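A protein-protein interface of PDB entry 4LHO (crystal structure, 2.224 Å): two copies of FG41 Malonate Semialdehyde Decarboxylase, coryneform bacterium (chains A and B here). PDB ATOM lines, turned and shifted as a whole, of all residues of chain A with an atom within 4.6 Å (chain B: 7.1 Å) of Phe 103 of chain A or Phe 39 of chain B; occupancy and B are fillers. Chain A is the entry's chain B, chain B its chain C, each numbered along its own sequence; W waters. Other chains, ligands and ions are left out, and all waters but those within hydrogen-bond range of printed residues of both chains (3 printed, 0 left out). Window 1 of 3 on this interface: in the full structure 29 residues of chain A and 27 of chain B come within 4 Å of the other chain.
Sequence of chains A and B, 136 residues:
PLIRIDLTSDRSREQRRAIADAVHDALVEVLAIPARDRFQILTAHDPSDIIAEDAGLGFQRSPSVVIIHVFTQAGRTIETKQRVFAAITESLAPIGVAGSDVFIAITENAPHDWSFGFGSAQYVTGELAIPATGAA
Of the printed residues of chain B, Glu 53 of chain A touches Arg 36 (3.2 Å), Arg 38 (2.9 Å) and Phe 39 (3.1 Å). Of the printed residues of chain B, Arg 61 of chain A touches Phe 39 (3.5 Å) and Phe 116 (2.7 Å). Ile 68 of chain A touches none of the printed residues of chain B. Phe 103 of chain A touches four residues of chain B. Printed residues of chain B within 4 Å of Ile 104 of chain A: Trp 114 and Ser 115. Asp 37 of chain B touches none of the printed residues of chain A. Printed residues of chain A within 4 Å of Phe 116 of chain B: Ala 55, Arg 61, Val 102 and Phe 103. The nearest residue of chain B that does not touch Phe 103 of chain A is Leu 2 of chain B (4.3 Å). The nearest residue of chain A that does not touch Phe 39 of chain B is Ala 55 of chain A (4.1 Å).
The backbone carbonyl oxygen of Ile 51 of chain A is in hydrogen-bond range of the backbone NH of Gln 40 of chain B. OE1 of Glu 53 of chain A is in salt-bridge range of NH1 of Arg 36 of chain B (3.6 Å). O of Arg 38 of chain B sits at hydrogen-bond distance from N of Glu 53 of chain A (2.9 Å). The backbone NH (N) of Ala 55 of chain A is in hydrogen-bond range of the backbone carbonyl oxygen (O) of Arg 36 of chain B (2.9 Å). The backbone carbonyl oxygen (O) of Phe 116 of chain B sits at hydrogen-bond distance from the guanidinium group (NH2) of Arg 61 of chain A (2.7 Å). The backbone NH (N) of Ile 104 of chain A sits at hydrogen-bond distance from the backbone carbonyl oxygen (O) of Ser 115 of chain B, 2.8 Å away. The backbone carbonyl oxygen (O) of Ile 51 of chain A sits close to the backbone carbonyl oxygen (O) of Arg 38 of chain B, 3.3 Å away.
Among the printed residues, pairs that only touch across the chains: Glu 53 of chain A with Phe 39 of chain B (3.1 Å), Val 102 of chain A with Gly 117 of chain B (3.2 Å), Ile 51 of chain A with Phe 39 of chain B (3.3 Å), Phe 103 of chain A with Phe 39 of chain B (3.3 Å), Ala 52 of chain A with Arg 38 of chain B (3.4 Å), Phe 103 of chain A with Ser 115 of chain B (3.4 Å), Arg 61 of chain A with Phe 39 of chain B (3.5 Å), Ile 104 of chain A with Trp 114 of chain B (3.6 Å), Ile 67 of chain A with Ile 41 of chain B (3.6 Å), Ala 105 of chain A with Trp 114 of chain B (3.7 Å), Phe 103 of chain A with Trp 114 of chain B (3.7 Å), Ala 52 of chain A with Phe 39 of chain B (3.8 Å), Phe 103 of chain A with Phe 116 of chain B (3.9 Å), Ala 55 of chain A with Phe 116 of chain B (3.9 Å) and Val 102 of chain A with Phe 116 of chain B (3.9 Å).
Printed residues of chain A that touch a printed residue of chain B: Ile 51, Ala 52, Glu 53, Ala 55, Arg 61, Ile 67, Val 102, Phe 103, Ile 104 and Ala 105. Hydrophobic or aromatic side chains of chain A within 4 Å of the printed part of chain B: Ile 51, Ala 52, Ala 55, Ile 67, Phe 103, Ile 104 and Ala 105. Among the printed residues, Asp or Glu carboxylates within 4 Å of a Lys or Arg side-chain nitrogen of the other chain: Glu 53 of chain A with Arg 36 of chain B (3.6 Å).
No position is printed for both chains. Of the 22 pairs that touch across the chains among the printed residues, none has its exchanged pair printed and touching as well.
Water W3 bridges the side-chain carboxylate (OE2) of Glu 53 of chain A and the guanidinium group (NH1) of Arg 38 of chain B. Water W1 lies within hydrogen-bond range of OG of Ser 115 of chain B (2.7 Å), O of Val 102 of chain A (3.1 Å), N of Phe 118 of chain B (3.3 Å) and N of Gly 117 of chain B (3.4 Å). Water W2 lies within hydrogen-bond range of the guanidinium group of Arg 4 of chain B and the backbone carbonyl oxygen of Ile 67 of chain A.
O of Ala 52 of chain A sits at hydrogen-bond distance from NE of Arg 61 of chain A, at 3.1 Å. The backbone NH of Phe 103 of chain A sits at hydrogen-bond distance from the backbone carbonyl oxygen of Val 66 of chain A (3.1 Å). N of Ile 68 of chain A lies within hydrogen-bond range of O of Phe 103 of chain A, at 2.9 Å. The backbone carbonyl oxygen (O) of Ile 68 of chain A lies within hydrogen-bond range of the backbone NH (N) of Ala 105 of chain A (2.9 Å). The backbone NH (N) of Ile 3 of chain B is in hydrogen-bond range of the backbone carbonyl oxygen (O) of Phe 39 of chain B, at 2.9 Å. The guanidinium group (NE) of Arg 38 of chain B lies within hydrogen-bond range of the side-chain amide oxygen (OE1) of Gln 40 of chain B.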
ATOM      1  N   ILE A  51      24.212 -27.875  13.284  1.00  0.00           N
ATOM      2  CA  ILE A  51      23.387 -29.044  13.527  1.00  0.00           C
ATOM      3  C   ILE A  51      22.059 -28.825  12.810  1.00  0.00           C
ATOM      4  O   ILE A  51      21.286 -27.987  13.204  1.00  0.00           O
ATOM      5  CB  ILE A  51      23.114 -29.238  15.017  1.00  0.00           C
ATOM      6  CG1 ILE A  51      24.432 -29.324  15.796  1.00  0.00           C
ATOM      7  CG2 ILE A  51      22.275 -30.493  15.257  1.00  0.00           C
ATOM      8  CD1 ILE A  51      24.254 -29.246  17.292  1.00  0.00           C
ATOM      9  N   ALA A  52      21.819 -29.559  11.736  1.00  0.00           N
ATOM     10  CA  ALA A  52      20.579 -29.396  10.980  1.00  0.00           C
ATOM     11  C   ALA A  52      20.029 -30.779  10.692  1.00  0.00           C
ATOM     12  O   ALA A  52      20.569 -31.507   9.854  1.00  0.00           O
ATOM     13  CB  ALA A  52      20.836 -28.635   9.686  1.00  0.00           C
ATOM     14  N   GLU A  53      18.996 -31.151  11.441  1.00  0.00           N
ATOM     15  CA  GLU A  53      18.373 -32.461  11.300  1.00  0.00           C
ATOM     16  C   GLU A  53      17.317 -32.362  10.177  1.00  0.00           C
ATOM     17  O   GLU A  53      17.419 -31.468   9.331  1.00  0.00           O
ATOM     18  CB  GLU A  53      17.819 -32.951  12.649  1.00  0.00           C
ATOM     19  CG  GLU A  53      18.943 -33.356  13.601  1.00  0.00           C
ATOM     20  CD  GLU A  53      18.492 -33.762  15.006  1.00  0.00           C
ATOM     21  OE1 GLU A  53      17.285 -33.911  15.270  1.00  0.00           O
ATOM     22  OE2 GLU A  53      19.374 -33.924  15.877  1.00  0.00           O
ATOM     23  N   ALA A  55      13.748 -32.578  10.393  1.00  0.00           N
ATOM     24  CA  ALA A  55      12.402 -32.152  10.749  1.00  0.00           C
ATOM     25  C   ALA A  55      11.384 -33.316  10.706  1.00  0.00           C
ATOM     26  O   ALA A  55      10.197 -33.106  10.567  1.00  0.00           O
ATOM     27  CB  ALA A  55      11.962 -31.012   9.838  1.00  0.00           C
ATOM     28  N   ARG A  61      21.315 -35.658   5.837  1.00  0.00           N
ATOM     29  CA  ARG A  61      22.210 -34.683   5.233  1.00  0.00           C
ATOM     30  C   ARG A  61      23.638 -35.175   5.446  1.00  0.00           C
ATOM     31  O   ARG A  61      23.884 -35.968   6.342  1.00  0.00           O
ATOM     32  CB  ARG A  61      22.041 -33.325   5.907  1.00  0.00           C
ATOM     33  CG  ARG A  61      20.606 -32.891   6.123  1.00  0.00           C
ATOM     34  CD  ARG A  61      20.534 -31.449   6.660  1.00  0.00           C
ATOM     35  NE  ARG A  61      19.198 -31.052   7.126  1.00  0.00           N
ATOM     36  CZ  ARG A  61      18.359 -30.281   6.430  1.00  0.00           C
ATOM     37  NH1 ARG A  61      18.677 -29.840   5.233  1.00  0.00           N
ATOM     38  NH2 ARG A  61      17.188 -29.957   6.917  1.00  0.00           N
ATOM     39  N   VAL A  66      24.674 -26.203   4.495  1.00  0.00           N
ATOM     40  CA  VAL A  66      24.772 -24.802   4.102  1.00  0.00           C
ATOM     41  C   VAL A  66      23.490 -24.121   4.495  1.00  0.00           C
ATOM     42  O   VAL A  66      22.438 -24.460   3.984  1.00  0.00           O
ATOM     43  CB  VAL A  66      24.977 -24.659   2.602  1.00  0.00           C
ATOM     44  CG1 VAL A  66      25.152 -23.183   2.217  1.00  0.00           C
ATOM     45  CG2 VAL A  66      26.181 -25.482   2.170  1.00  0.00           C
ATOM     46  N   ILE A  67      23.577 -23.184   5.438  1.00  0.00           N
ATOM     47  CA  ILE A  67      22.416 -22.446   5.899  1.00  0.00           C
ATOM     48  C   ILE A  67      22.429 -21.047   5.291  1.00  0.00           C
ATOM     49  O   ILE A  67      23.403 -20.323   5.377  1.00  0.00           O
ATOM     50  CB  ILE A  67      22.336 -22.413   7.424  1.00  0.00           C
ATOM     51  CG1 ILE A  67      22.091 -23.839   7.937  1.00  0.00           C
ATOM     52  CG2 ILE A  67      21.226 -21.495   7.877  1.00  0.00           C
ATOM     53  CD1 ILE A  67      22.288 -23.993   9.398  1.00  0.00           C
ATOM     54  N   ILE A  68      21.328 -20.699   4.633  1.00  0.00           N
ATOM     55  CA  ILE A  68      21.210 -19.444   3.916  1.00  0.00           C
ATOM     56  C   ILE A  68      20.056 -18.651   4.544  1.00  0.00           C
ATOM     57  O   ILE A  68      18.906 -19.088   4.557  1.00  0.00           O
ATOM     58  CB  ILE A  68      20.962 -19.696   2.429  1.00  0.00           C
ATOM     59  CG1 ILE A  68      22.187 -20.372   1.786  1.00  0.00           C
ATOM     60  CG2 ILE A  68      20.670 -18.392   1.709  1.00  0.00           C
ATOM     61  CD1 ILE A  68      21.869 -21.019   0.472  1.00  0.00           C
ATOM     62  N   ASP A 101      21.345 -30.895   1.724  1.00  0.00           N
ATOM     63  CA  ASP A 101      22.243 -30.149   2.590  1.00  0.00           C
ATOM     64  C   ASP A 101      21.961 -28.622   2.653  1.00  0.00           C
ATOM     65  O   ASP A 101      22.700 -27.906   3.298  1.00  0.00           O
ATOM     66  CB  ASP A 101      23.689 -30.384   2.149  1.00  0.00           C
ATOM     67  CG  ASP A 101      24.106 -31.823   2.284  1.00  0.00           C
ATOM     68  OD1 ASP A 101      23.393 -32.591   2.956  1.00  0.00           O
ATOM     69  OD2 ASP A 101      25.150 -32.183   1.711  1.00  0.00           O
ATOM     70  N   VAL A 102      20.921 -28.142   1.970  1.00  0.00           N
ATOM     71  CA  VAL A 102      20.592 -26.717   1.944  1.00  0.00           C
ATOM     72  C   VAL A 102      19.378 -26.352   2.837  1.00  0.00           C
ATOM     73  O   VAL A 102      18.332 -26.962   2.740  1.00  0.00           O
ATOM     74  CB  VAL A 102      20.250 -26.283   0.523  1.00  0.00           C
ATOM     75  CG1 VAL A 102      19.972 -24.777   0.490  1.00  0.00           C
ATOM     76  CG2 VAL A 102      21.350 -26.661  -0.430  1.00  0.00           C
ATOM     77  N   PHE A 103      19.523 -25.354   3.699  1.00  0.00           N
ATOM     78  CA  PHE A 103      18.442 -24.944   4.604  1.00  0.00           C
ATOM     79  C   PHE A 103      18.288 -23.439   4.378  1.00  0.00           C
ATOM     80  O   PHE A 103      19.288 -22.729   4.318  1.00  0.00           O
ATOM     81  CB  PHE A 103      18.792 -25.328   6.058  1.00  0.00           C
ATOM     82  CG  PHE A 103      17.791 -24.891   7.064  1.00  0.00           C
ATOM     83  CD1 PHE A 103      16.903 -25.789   7.618  1.00  0.00           C
ATOM     84  CD2 PHE A 103      17.726 -23.572   7.459  1.00  0.00           C
ATOM     85  CE1 PHE A 103      15.950 -25.379   8.538  1.00  0.00           C
ATOM     86  CE2 PHE A 103      16.769 -23.156   8.384  1.00  0.00           C
ATOM     87  CZ  PHE A 103      15.881 -24.059   8.916  1.00  0.00           C
ATOM     88  N   ILE A 104      17.069 -22.954   4.142  1.00  0.00           N
ATOM     89  CA  ILE A 104      16.904 -21.541   3.790  1.00  0.00           C
ATOM     90  C   ILE A 104      15.852 -20.894   4.670  1.00  0.00           C
ATOM     91  O   ILE A 104      14.802 -21.495   4.963  1.00  0.00           O
ATOM     92  CB  ILE A 104      16.540 -21.342   2.314  1.00  0.00           C
ATOM     93  CG1 ILE A 104      17.439 -22.191   1.432  1.00  0.00           C
ATOM     94  CG2 ILE A 104      16.640 -19.846   1.904  1.00  0.00           C
ATOM     95  CD1 ILE A 104      17.095 -22.108  -0.050  1.00  0.00           C
ATOM     96  N   ALA A 105      16.158 -19.685   5.144  1.00  0.00           N
ATOM     97  CA  ALA A 105      15.186 -18.920   5.947  1.00  0.00           C
ATOM     98  C   ALA A 105      15.088 -17.478   5.462  1.00  0.00           C
ATOM     99  O   ALA A 105      16.072 -16.917   5.023  1.00  0.00           O
ATOM    100  CB  ALA A 105      15.552 -18.942   7.402  1.00  0.00           C
ATOM    101  N   PRO B   1      12.440 -23.981  14.289  1.00  0.00           N
ATOM    102  CA  PRO B   1      13.078 -22.666  14.418  1.00  0.00           C
ATOM    103  C   PRO B   1      14.572 -22.795  14.146  1.00  0.00           C
ATOM    104  O   PRO B   1      15.121 -23.891  14.225  1.00  0.00           O
ATOM    105  CB  PRO B   1      12.844 -22.312  15.883  1.00  0.00           C
ATOM    106  CG  PRO B   1      12.757 -23.615  16.586  1.00  0.00           C
ATOM    107  CD  PRO B   1      12.140 -24.602  15.593  1.00  0.00           C
ATOM    108  N   LEU B   2      15.213 -21.686  13.811  1.00  0.00           N
ATOM    109  CA  LEU B   2      16.627 -21.657  13.535  1.00  0.00           C
ATOM    110  C   LEU B   2      17.219 -20.892  14.715  1.00  0.00           C
ATOM    111  O   LEU B   2      16.782 -19.787  15.003  1.00  0.00           O
ATOM    112  CB  LEU B   2      16.915 -20.943  12.204  1.00  0.00           C
ATOM    113  CG  LEU B   2      18.393 -20.635  11.953  1.00  0.00           C
ATOM    114  CD1 LEU B   2      19.186 -21.915  11.776  1.00  0.00           C
ATOM    115  CD2 LEU B   2      18.589 -19.709  10.756  1.00  0.00           C
ATOM    116  N   ILE B   3      18.171 -21.515  15.400  1.00  0.00           N
ATOM    117  CA  ILE B   3      18.718 -21.001  16.639  1.00  0.00           C
ATOM    118  C   ILE B   3      20.155 -20.650  16.404  1.00  0.00           C
ATOM    119  O   ILE B   3      20.912 -21.512  16.017  1.00  0.00           O
ATOM    120  CB  ILE B   3      18.707 -22.052  17.737  1.00  0.00           C
ATOM    121  CG1 ILE B   3      17.362 -22.797  17.743  1.00  0.00           C
ATOM    122  CG2 ILE B   3      18.994 -21.386  19.054  1.00  0.00           C
ATOM    123  CD1 ILE B   3      16.169 -21.920  17.999  1.00  0.00           C
ATOM    124  N   ARG B   4      20.512 -19.376  16.565  1.00  0.00           N
ATOM    125  CA  ARG B   4      21.919 -18.958  16.542  1.00  0.00           C
ATOM    126  C   ARG B   4      22.382 -18.860  18.003  1.00  0.00           C
ATOM    127  O   ARG B   4      21.802 -18.113  18.836  1.00  0.00           O
ATOM    128  CB  ARG B   4      22.116 -17.611  15.828  1.00  0.00           C
ATOM    129  CG  ARG B   4      21.874 -17.658  14.365  1.00  0.00           C
ATOM    130  CD  ARG B   4      22.240 -16.363  13.641  1.00  0.00           C
ATOM    131  NE  ARG B   4      21.727 -16.481  12.276  1.00  0.00           N
ATOM    132  CZ  ARG B   4      22.437 -16.847  11.213  1.00  0.00           C
ATOM    133  NH1 ARG B   4      23.761 -17.068  11.293  1.00  0.00           N
ATOM    134  NH2 ARG B   4      21.818 -16.961  10.055  1.00  0.00           N
ATOM    135  N   HIS B  24      17.854 -27.104  22.714  1.00  0.00           N
ATOM    136  CA  HIS B  24      16.970 -27.907  21.893  1.00  0.00           C
ATOM    137  C   HIS B  24      15.925 -28.619  22.743  1.00  0.00           C
ATOM    138  O   HIS B  24      14.748 -28.564  22.413  1.00  0.00           O
ATOM    139  CB  HIS B  24      17.736 -28.897  21.029  1.00  0.00           C
ATOM    140  CG  HIS B  24      16.840 -29.698  20.138  1.00  0.00           C
ATOM    141  ND1 HIS B  24      16.076 -29.122  19.140  1.00  0.00           N
ATOM    142  CD2 HIS B  24      16.537 -31.016  20.135  1.00  0.00           C
ATOM    143  CE1 HIS B  24      15.351 -30.058  18.556  1.00  0.00           C
ATOM    144  NE2 HIS B  24      15.608 -31.213  19.143  1.00  0.00           N
ATOM    145  N   LEU B  27      13.226 -26.251  23.908  1.00  0.00           N
ATOM    146  CA  LEU B  27      12.263 -25.780  22.929  1.00  0.00           C
ATOM    147  C   LEU B  27      11.265 -26.896  22.628  1.00  0.00           C
ATOM    148  O   LEU B  27      10.077 -26.657  22.541  1.00  0.00           O
ATOM    149  CB  LEU B  27      12.959 -25.316  21.644  1.00  0.00           C
ATOM    150  CG  LEU B  27      13.825 -24.065  21.718  1.00  0.00           C
ATOM    151  CD1 LEU B  27      14.608 -23.856  20.425  1.00  0.00           C
ATOM    152  CD2 LEU B  27      13.008 -22.828  22.068  1.00  0.00           C
ATOM    153  N   ARG B  36      13.128 -33.703  15.927  1.00  0.00           N
ATOM    154  CA  ARG B  36      14.129 -33.596  14.893  1.00  0.00           C
ATOM    155  C   ARG B  36      14.023 -32.260  14.134  1.00  0.00           C
ATOM    156  O   ARG B  36      14.693 -32.039  13.121  1.00  0.00           O
ATOM    157  CB  ARG B  36      14.063 -34.802  13.975  1.00  0.00           C
ATOM    158  CG  ARG B  36      14.614 -36.059  14.642  1.00  0.00           C
ATOM    159  CD  ARG B  36      14.904 -37.204  13.662  1.00  0.00           C
ATOM    160  NE  ARG B  36      15.771 -36.798  12.553  1.00  0.00           N
ATOM    161  CZ  ARG B  36      17.110 -36.753  12.581  1.00  0.00           C
ATOM    162  NH1 ARG B  36      17.775 -37.110  13.684  1.00  0.00           N
ATOM    163  NH2 ARG B  36      17.793 -36.337  11.496  1.00  0.00           N
ATOM    164  N   ASP B  37      13.197 -31.358  14.655  1.00  0.00           N
ATOM    165  CA  ASP B  37      13.156 -29.986  14.152  1.00  0.00           C
ATOM    166  C   ASP B  37      14.305 -29.154  14.809  1.00  0.00           C
ATOM    167  O   ASP B  37      14.087 -28.201  15.553  1.00  0.00           O
ATOM    168  CB  ASP B  37      11.771 -29.423  14.438  1.00  0.00           C
ATOM    169  CG  ASP B  37      11.569 -28.071  13.880  1.00  0.00           C
ATOM    170  OD1 ASP B  37      12.397 -27.631  13.052  1.00  0.00           O
ATOM    171  OD2 ASP B  37      10.568 -27.442  14.279  1.00  0.00           O
ATOM    172  N   ARG B  38      15.534 -29.571  14.528  1.00  0.00           N
ATOM    173  CA  ARG B  38      16.709 -29.063  15.196  1.00  0.00           C
ATOM    174  C   ARG B  38      17.623 -28.419  14.187  1.00  0.00           C
ATOM    175  O   ARG B  38      18.231 -29.090  13.359  1.00  0.00           O
ATOM    176  CB  ARG B  38      17.434 -30.192  15.938  1.00  0.00           C
ATOM    177  CG  ARG B  38      18.603 -29.690  16.739  1.00  0.00           C
ATOM    178  CD  ARG B  38      19.290 -30.756  17.582  1.00  0.00           C
ATOM    179  NE  ARG B  38      20.316 -30.124  18.428  1.00  0.00           N
ATOM    180  CZ  ARG B  38      20.943 -30.693  19.454  1.00  0.00           C
ATOM    181  NH1 ARG B  38      20.718 -31.953  19.814  1.00  0.00           N
ATOM    182  NH2 ARG B  38      21.833 -29.993  20.108  1.00  0.00           N
ATOM    183  N   PHE B  39      17.660 -27.099  14.232  1.00  0.00           N
ATOM    184  CA  PHE B  39      18.505 -26.309  13.339  1.00  0.00           C
ATOM    185  C   PHE B  39      19.243 -25.241  14.147  1.00  0.00           C
ATOM    186  O   PHE B  39      18.621 -24.305  14.688  1.00  0.00           O
ATOM    187  CB  PHE B  39      17.619 -25.691  12.255  1.00  0.00           C
ATOM    188  CG  PHE B  39      16.768 -26.711  11.599  1.00  0.00           C
ATOM    189  CD1 PHE B  39      15.502 -26.933  12.010  1.00  0.00           C
ATOM    190  CD2 PHE B  39      17.317 -27.544  10.658  1.00  0.00           C
ATOM    191  CE1 PHE B  39      14.764 -27.927  11.419  1.00  0.00           C
ATOM    192  CE2 PHE B  39      16.586 -28.528  10.094  1.00  0.00           C
ATOM    193  CZ  PHE B  39      15.310 -28.716  10.477  1.00  0.00           C
ATOM    194  N   GLN B  40      20.553 -25.421  14.255  1.00  0.00           N
ATOM    195  CA  GLN B  40      21.387 -24.604  15.136  1.00  0.00           C
ATOM    196  C   GLN B  40      22.727 -24.296  14.530  1.00  0.00           C
ATOM    197  O   GLN B  40      23.380 -25.152  13.957  1.00  0.00           O
ATOM    198  CB  GLN B  40      21.585 -25.287  16.492  1.00  0.00           C
ATOM    199  CG  GLN B  40      20.293 -25.752  17.177  1.00  0.00           C
ATOM    200  CD  GLN B  40      20.563 -26.546  18.468  1.00  0.00           C
ATOM    201  OE1 GLN B  40      21.450 -27.393  18.511  1.00  0.00           O
ATOM    202  NE2 GLN B  40      19.818 -26.253  19.513  1.00  0.00           N
ATOM    203  N   ILE B  41      23.131 -23.040  14.681  1.00  0.00           N
ATOM    204  CA  ILE B  41      24.453 -22.590  14.322  1.00  0.00           C
ATOM    205  C   ILE B  41      25.141 -22.099  15.608  1.00  0.00           C
ATOM    206  O   ILE B  41      24.728 -21.126  16.228  1.00  0.00           O
ATOM    207  CB  ILE B  41      24.375 -21.448  13.278  1.00  0.00           C
ATOM    208  CG1 ILE B  41      23.552 -21.917  12.067  1.00  0.00           C
ATOM    209  CG2 ILE B  41      25.765 -21.004  12.819  1.00  0.00           C
ATOM    210  CD1 ILE B  41      23.123 -20.795  11.157  1.00  0.00           C
ATOM    211  N   PHE B  71      15.097 -17.719  15.771  1.00  0.00           N
ATOM    212  CA  PHE B  71      14.259 -17.357  14.635  1.00  0.00           C
ATOM    213  C   PHE B  71      13.174 -18.378  14.432  1.00  0.00           C
ATOM    214  O   PHE B  71      13.447 -19.514  14.058  1.00  0.00           O
ATOM    215  CB  PHE B  71      15.083 -17.254  13.380  1.00  0.00           C
ATOM    216  CG  PHE B  71      16.076 -16.173  13.429  1.00  0.00           C
ATOM    217  CD1 PHE B  71      15.779 -14.938  12.899  1.00  0.00           C
ATOM    218  CD2 PHE B  71      17.315 -16.375  14.036  1.00  0.00           C
ATOM    219  CE1 PHE B  71      16.721 -13.909  12.945  1.00  0.00           C
ATOM    220  CE2 PHE B  71      18.245 -15.353  14.077  1.00  0.00           C
ATOM    221  CZ  PHE B  71      17.931 -14.110  13.531  1.00  0.00           C
ATOM    222  N   TRP B 114      10.319 -20.519   5.072  1.00  0.00           N
ATOM    223  CA  TRP B 114      11.222 -21.631   5.405  1.00  0.00           C
ATOM    224  C   TRP B 114      11.393 -22.663   4.290  1.00  0.00           C
ATOM    225  O   TRP B 114      10.412 -23.153   3.722  1.00  0.00           O
ATOM    226  CB  TRP B 114      10.740 -22.365   6.675  1.00  0.00           C
ATOM    227  CG  TRP B 114      10.694 -21.477   7.870  1.00  0.00           C
ATOM    228  CD1 TRP B 114       9.630 -20.765   8.312  1.00  0.00           C
ATOM    229  CD2 TRP B 114      11.773 -21.181   8.765  1.00  0.00           C
ATOM    230  NE1 TRP B 114       9.974 -20.026   9.417  1.00  0.00           N
ATOM    231  CE2 TRP B 114      11.283 -20.272   9.723  1.00  0.00           C
ATOM    232  CE3 TRP B 114      13.102 -21.580   8.837  1.00  0.00           C
ATOM    233  CZ2 TRP B 114      12.080 -19.773  10.767  1.00  0.00           C
ATOM    234  CZ3 TRP B 114      13.891 -21.089   9.869  1.00  0.00           C
ATOM    235  CH2 TRP B 114      13.376 -20.196  10.820  1.00  0.00           C
ATOM    236  N   SER B 115      12.642 -23.015   4.011  1.00  0.00           N
ATOM    237  CA  SER B 115      12.949 -24.221   3.262  1.00  0.00           C
ATOM    238  C   SER B 115      13.869 -25.168   4.050  1.00  0.00           C
ATOM    239  O   SER B 115      15.030 -24.845   4.284  1.00  0.00           O
ATOM    240  CB  SER B 115      13.618 -23.877   1.939  1.00  0.00           C
ATOM    241  OG  SER B 115      13.803 -25.078   1.179  1.00  0.00           O
ATOM    242  N   PHE B 116      13.364 -26.352   4.400  1.00  0.00           N
ATOM    243  CA  PHE B 116      14.119 -27.325   5.179  1.00  0.00           C
ATOM    244  C   PHE B 116      15.000 -28.220   4.323  1.00  0.00           C
ATOM    245  O   PHE B 116      15.750 -29.027   4.844  1.00  0.00           O
ATOM    246  CB  PHE B 116      13.200 -28.197   6.020  1.00  0.00           C
ATOM    247  CG  PHE B 116      12.414 -27.432   7.038  1.00  0.00           C
ATOM    248  CD1 PHE B 116      12.736 -27.495   8.369  1.00  0.00           C
ATOM    249  CD2 PHE B 116      11.357 -26.632   6.657  1.00  0.00           C
ATOM    250  CE1 PHE B 116      12.023 -26.781   9.317  1.00  0.00           C
ATOM    251  CE2 PHE B 116      10.635 -25.923   7.609  1.00  0.00           C
ATOM    252  CZ  PHE B 116      10.980 -26.007   8.946  1.00  0.00           C
ATOM    253  N   GLY B 117      14.934 -28.068   3.012  1.00  0.00           N
ATOM    254  CA  GLY B 117      15.797 -28.832   2.141  1.00  0.00           C
ATOM    255  C   GLY B 117      15.152 -29.060   0.788  1.00  0.00           C
ATOM    256  O   GLY B 117      13.938 -28.894   0.641  1.00  0.00           O
ATOM    257  N   PHE B 118      15.988 -29.382  -0.197  1.00  0.00           N
ATOM    258  CA  PHE B 118      15.537 -29.797  -1.519  1.00  0.00           C
ATOM    259  C   PHE B 118      14.857 -28.663  -2.304  1.00  0.00           C
ATOM    260  O   PHE B 118      14.218 -28.889  -3.351  1.00  0.00           O
ATOM    261  CB  PHE B 118      14.622 -31.025  -1.387  1.00  0.00           C
ATOM    262  CG  PHE B 118      15.256 -32.154  -0.672  1.00  0.00           C
ATOM    263  CD1 PHE B 118      16.379 -32.780  -1.195  1.00  0.00           C
ATOM    264  CD2 PHE B 118      14.748 -32.588   0.540  1.00  0.00           C
ATOM    265  CE1 PHE B 118      16.985 -33.835  -0.504  1.00  0.00           C
ATOM    266  CE2 PHE B 118      15.324 -33.638   1.230  1.00  0.00           C
ATOM    267  CZ  PHE B 118      16.440 -34.282   0.703  1.00  0.00           C
ATOM    268  N   TYR B 123       6.231 -26.210   4.502  1.00  0.00           N
ATOM    269  CA  TYR B 123       4.994 -25.807   5.158  1.00  0.00           C
ATOM    270  C   TYR B 123       3.985 -25.360   4.089  1.00  0.00           C
ATOM    271  O   TYR B 123       2.792 -25.529   4.268  1.00  0.00           O
ATOM    272  CB  TYR B 123       5.182 -24.654   6.157  1.00  0.00           C
ATOM    273  CG  TYR B 123       5.891 -25.002   7.435  1.00  0.00           C
ATOM    274  CD1 TYR B 123       5.462 -26.034   8.263  1.00  0.00           C
ATOM    275  CD2 TYR B 123       7.031 -24.309   7.789  1.00  0.00           C
ATOM    276  CE1 TYR B 123       6.150 -26.344   9.429  1.00  0.00           C
ATOM    277  CE2 TYR B 123       7.717 -24.600   8.931  1.00  0.00           C
ATOM    278  CZ  TYR B 123       7.288 -25.609   9.755  1.00  0.00           C
ATOM    279  OH  TYR B 123       8.034 -25.831  10.889  1.00  0.00           O
HETATM  280  O   HOH W   1      16.244 -26.141   0.586  1.00  0.00           O
HETATM  281  O   HOH W   2      23.048 -18.228   7.959  1.00  0.00           O
HETATM  282  O   HOH W   3      18.821 -34.111  18.450  1.00  0.00           O
